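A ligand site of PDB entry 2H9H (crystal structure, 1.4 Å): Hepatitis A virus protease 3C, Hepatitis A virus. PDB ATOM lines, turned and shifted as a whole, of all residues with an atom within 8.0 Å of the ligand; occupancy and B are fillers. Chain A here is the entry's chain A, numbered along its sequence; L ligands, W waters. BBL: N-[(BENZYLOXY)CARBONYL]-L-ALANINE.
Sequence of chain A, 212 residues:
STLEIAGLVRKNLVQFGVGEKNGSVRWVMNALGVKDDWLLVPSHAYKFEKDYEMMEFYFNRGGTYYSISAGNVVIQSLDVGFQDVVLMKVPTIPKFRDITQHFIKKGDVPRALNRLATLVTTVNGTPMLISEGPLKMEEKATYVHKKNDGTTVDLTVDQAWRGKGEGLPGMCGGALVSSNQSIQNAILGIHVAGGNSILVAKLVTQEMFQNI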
ATOM      1  N   GLU A   4      -0.951  25.157 -13.067  1.00  0.00           N
ATOM      2  CA  GLU A   4      -1.000  25.567 -11.652  1.00  0.00           C
ATOM      3  C   GLU A   4      -0.086  24.710 -10.752  1.00  0.00           C
ATOM      4  O   GLU A   4       0.599  25.244  -9.877  1.00  0.00           O
ATOM      5  CB  GLU A   4      -2.437  25.634 -11.109  1.00  0.00           C
ATOM      6  CG  GLU A   4      -3.307  26.701 -11.783  1.00  0.00           C
ATOM      7  CD  GLU A   4      -2.905  28.145 -11.468  1.00  0.00           C
ATOM      8  OE1 GLU A   4      -2.277  28.380 -10.425  1.00  0.00           O
ATOM      9  OE2 GLU A   4      -3.244  29.050 -12.272  1.00  0.00           O
ATOM     10  N   ILE A   5      -0.049  23.404 -10.982  1.00  0.00           N
ATOM     11  CA  ILE A   5       0.972  22.571 -10.312  1.00  0.00           C
ATOM     12  C   ILE A   5       2.374  23.081 -10.681  1.00  0.00           C
ATOM     13  O   ILE A   5       3.238  23.186  -9.807  1.00  0.00           O
ATOM     14  CB  ILE A   5       0.852  21.074 -10.689  1.00  0.00           C
ATOM     15  CG1 ILE A   5      -0.451  20.495 -10.121  1.00  0.00           C
ATOM     16  CG2 ILE A   5       2.118  20.291 -10.217  1.00  0.00           C
ATOM     17  CD1 ILE A   5      -0.527  20.391  -8.607  1.00  0.00           C
ATOM     18  N   LEU A   8       3.430  25.952  -8.552  1.00  0.00           N
ATOM     19  CA  LEU A   8       3.813  25.521  -7.194  1.00  0.00           C
ATOM     20  C   LEU A   8       5.197  24.900  -7.178  1.00  0.00           C
ATOM     21  O   LEU A   8       5.966  25.108  -6.235  1.00  0.00           O
ATOM     22  CB  LEU A   8       2.803  24.536  -6.625  1.00  0.00           C
ATOM     23  CG  LEU A   8       1.360  25.008  -6.467  1.00  0.00           C
ATOM     24  CD1 LEU A   8       0.534  23.847  -5.972  1.00  0.00           C
ATOM     25  CD2 LEU A   8       1.259  26.178  -5.524  1.00  0.00           C
ATOM     26  N   ARG A  97       6.757  26.094   1.167  1.00  0.00           N
ATOM     27  CA  ARG A  97       5.373  25.661   1.090  1.00  0.00           C
ATOM     28  C   ARG A  97       5.376  24.137   0.987  1.00  0.00           C
ATOM     29  O   ARG A  97       6.139  23.575   0.178  1.00  0.00           O
ATOM     30  CB  ARG A  97       4.716  26.228  -0.161  1.00  0.00           C
ATOM     31  CG  ARG A  97       3.267  25.850  -0.335  1.00  0.00           C
ATOM     32  CD  ARG A  97       2.741  26.431  -1.620  1.00  0.00           C
ATOM     33  NE  ARG A  97       1.317  26.148  -1.788  1.00  0.00           N
ATOM     34  CZ  ARG A  97       0.466  26.982  -2.383  1.00  0.00           C
ATOM     35  NH1 ARG A  97       0.893  28.149  -2.873  1.00  0.00           N
ATOM     36  NH2 ARG A  97      -0.815  26.638  -2.498  1.00  0.00           N
ATOM     37  N   ASP A  98       4.563  23.492   1.815  1.00  0.00           N
ATOM     38  CA  ASP A  98       4.389  22.037   1.796  1.00  0.00           C
ATOM     39  C   ASP A  98       3.670  21.641   0.517  1.00  0.00           C
ATOM     40  O   ASP A  98       2.477  21.936   0.355  1.00  0.00           O
ATOM     41  CB  ASP A  98       3.597  21.589   3.019  1.00  0.00           C
ATOM     42  CG  ASP A  98       3.449  20.072   3.113  1.00  0.00           C
ATOM     43  OD1 ASP A  98       3.872  19.354   2.175  1.00  0.00           O
ATOM     44  OD2 ASP A  98       2.905  19.602   4.133  1.00  0.00           O
ATOM     45  N   ILE A  99       4.401  21.007  -0.395  1.00  0.00           N
ATOM     46  CA  ILE A  99       3.798  20.510  -1.646  1.00  0.00           C
ATOM     47  C   ILE A  99       3.723  18.991  -1.704  1.00  0.00           C
ATOM     48  O   ILE A  99       3.442  18.416  -2.757  1.00  0.00           O
ATOM     49  CB  ILE A  99       4.501  21.063  -2.930  1.00  0.00           C
ATOM     50  CG1 ILE A  99       5.998  20.723  -2.971  1.00  0.00           C
ATOM     51  CG2 ILE A  99       4.271  22.589  -3.060  1.00  0.00           C
ATOM     52  CD1 ILE A  99       6.662  20.934  -4.319  1.00  0.00           C
ATOM     53  N   THR A 100       3.980  18.338  -0.561  1.00  0.00           N
ATOM     54  CA  THR A 100       3.959  16.866  -0.504  1.00  0.00           C
ATOM     55  C   THR A 100       2.632  16.218  -0.944  1.00  0.00           C
ATOM     56  O   THR A 100       2.634  15.142  -1.552  1.00  0.00           O
ATOM     57  CB  THR A 100       4.375  16.312   0.884  1.00  0.00           C
ATOM     58  OG1 THR A 100       3.443  16.767   1.880  1.00  0.00           O
ATOM     59  CG2 THR A 100       5.795  16.735   1.260  1.00  0.00           C
ATOM     60  N   GLN A 101       1.517  16.872  -0.637  1.00  0.00           N
ATOM     61  CA  GLN A 101       0.187  16.320  -1.000  1.00  0.00           C
ATOM     62  C   GLN A 101      -0.118  16.369  -2.491  1.00  0.00           C
ATOM     63  O   GLN A 101      -1.144  15.819  -2.939  1.00  0.00           O
ATOM     64  CB  GLN A 101      -0.929  17.016  -0.200  1.00  0.00           C
ATOM     65  CG  GLN A 101      -0.743  16.907   1.310  1.00  0.00           C
ATOM     66  CD  GLN A 101      -0.494  15.488   1.774  1.00  0.00           C
ATOM     67  OE1 GLN A 101       0.615  15.144   2.178  1.00  0.00           O
ATOM     68  NE2 GLN A 101      -1.520  14.643   1.687  1.00  0.00           N
ATOM     69  N   HIS A 102       0.752  17.036  -3.251  1.00  0.00           N
ATOM     70  CA  HIS A 102       0.607  17.130  -4.702  1.00  0.00           C
ATOM     71  C   HIS A 102       1.395  16.043  -5.423  1.00  0.00           C
ATOM     72  O   HIS A 102       1.330  15.960  -6.647  1.00  0.00           O
ATOM     73  CB  HIS A 102       1.018  18.523  -5.221  1.00  0.00           C
ATOM     74  CG  HIS A 102       0.069  19.604  -4.793  1.00  0.00           C
ATOM     75  ND1 HIS A 102      -1.222  19.675  -5.291  1.00  0.00           N
ATOM     76  CD2 HIS A 102       0.199  20.637  -3.926  1.00  0.00           C
ATOM     77  CE1 HIS A 102      -1.844  20.700  -4.732  1.00  0.00           C
ATOM     78  NE2 HIS A 102      -1.011  21.311  -3.915  1.00  0.00           N
HETATM   79  OG2 BBL L   1      -1.035  24.469  -1.120  1.00  0.00           O
HETATM   80  CB2 BBL L   1      -1.946  23.605  -1.076  1.00  0.00           C
HETATM   81  OG1 BBL L   1      -2.991  23.781  -0.385  1.00  0.00           O
HETATM   82  CA  BBL L   1      -1.741  22.318  -1.843  1.00  0.00           C
HETATM   83  CBZ BBL L   1      -1.296  22.515  -3.302  1.00  0.00           C
HETATM   84  N   BBL L   1      -2.927  21.476  -1.800  1.00  0.00           N
HETATM   85  C   BBL L   1      -3.095  20.557  -0.860  1.00  0.00           C
HETATM   86  O   BBL L   1      -2.300  20.315   0.048  1.00  0.00           O
HETATM   87  OEZ BBL L   1      -4.329  19.806  -0.956  1.00  0.00           O
HETATM   88  CB  BBL L   1      -4.904  19.172   0.195  1.00  0.00           C
HETATM   89  CG  BBL L   1      -6.400  19.118   0.050  1.00  0.00           C
HETATM   90  CD1 BBL L   1      -7.111  18.127   0.712  1.00  0.00           C
HETATM   91  CE1 BBL L   1      -8.501  18.069   0.578  1.00  0.00           C
HETATM   92  CZ  BBL L   1      -9.156  18.999  -0.211  1.00  0.00           C
HETATM   93  CE2 BBL L   1      -8.443  19.993  -0.886  1.00  0.00           C
HETATM   94  CD2 BBL L   1      -7.060  20.049  -0.759  1.00  0.00           C
HETATM   95  O   HOH W   1      -2.456  26.382   0.293  1.00  0.00           O
HETATM   96  O   HOH W   2       0.694  23.472   1.608  1.00  0.00           O
HETATM   97  O   HOH W   3       0.786  19.657   0.132  1.00  0.00           O
HETATM   98  O   HOH W   4       1.355  23.329  -1.511  1.00  0.00           O
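OG1 of Thr 100 lies within hydrogen-bond range of OE1 of Gln 101, at 3.3 Å.
CD1 of Leu 8 touches CBZ of the ligand, at 3.5 Å.
Gln 101 touches the ligand (CB to O, 3.6 Å).
Water W4 lies within hydrogen-bond range of the backbone carbonyl oxygen of Asp 98, an oxygen (OG2) of the ligand and the guanidinium group of Arg 97.
Water W1 bridges an oxygen (OG1) of the ligand (2.7 Å) and the guanidinium group (NH2) of Arg 97 (3.2 Å).
Water W3 lies within hydrogen-bond range of the backbone carbonyl oxygen of Asp 98 (2.8 Å), the backbone NH of Gln 101 (3.0 Å) and an oxygen (O) of the ligand (3.2 Å).
Water W2 lies within hydrogen-bond range of the backbone carbonyl oxygen of Asp 98 and an oxygen (OG2) of the ligand.
A ring nitrogen (NE2) of His 102 is covalently linked to a carbon (CBZ) of the ligand (1.4 Å).
NH2 of Arg 97 lies within salt-bridge range of OG2 of the ligand, at 2.6 Å.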
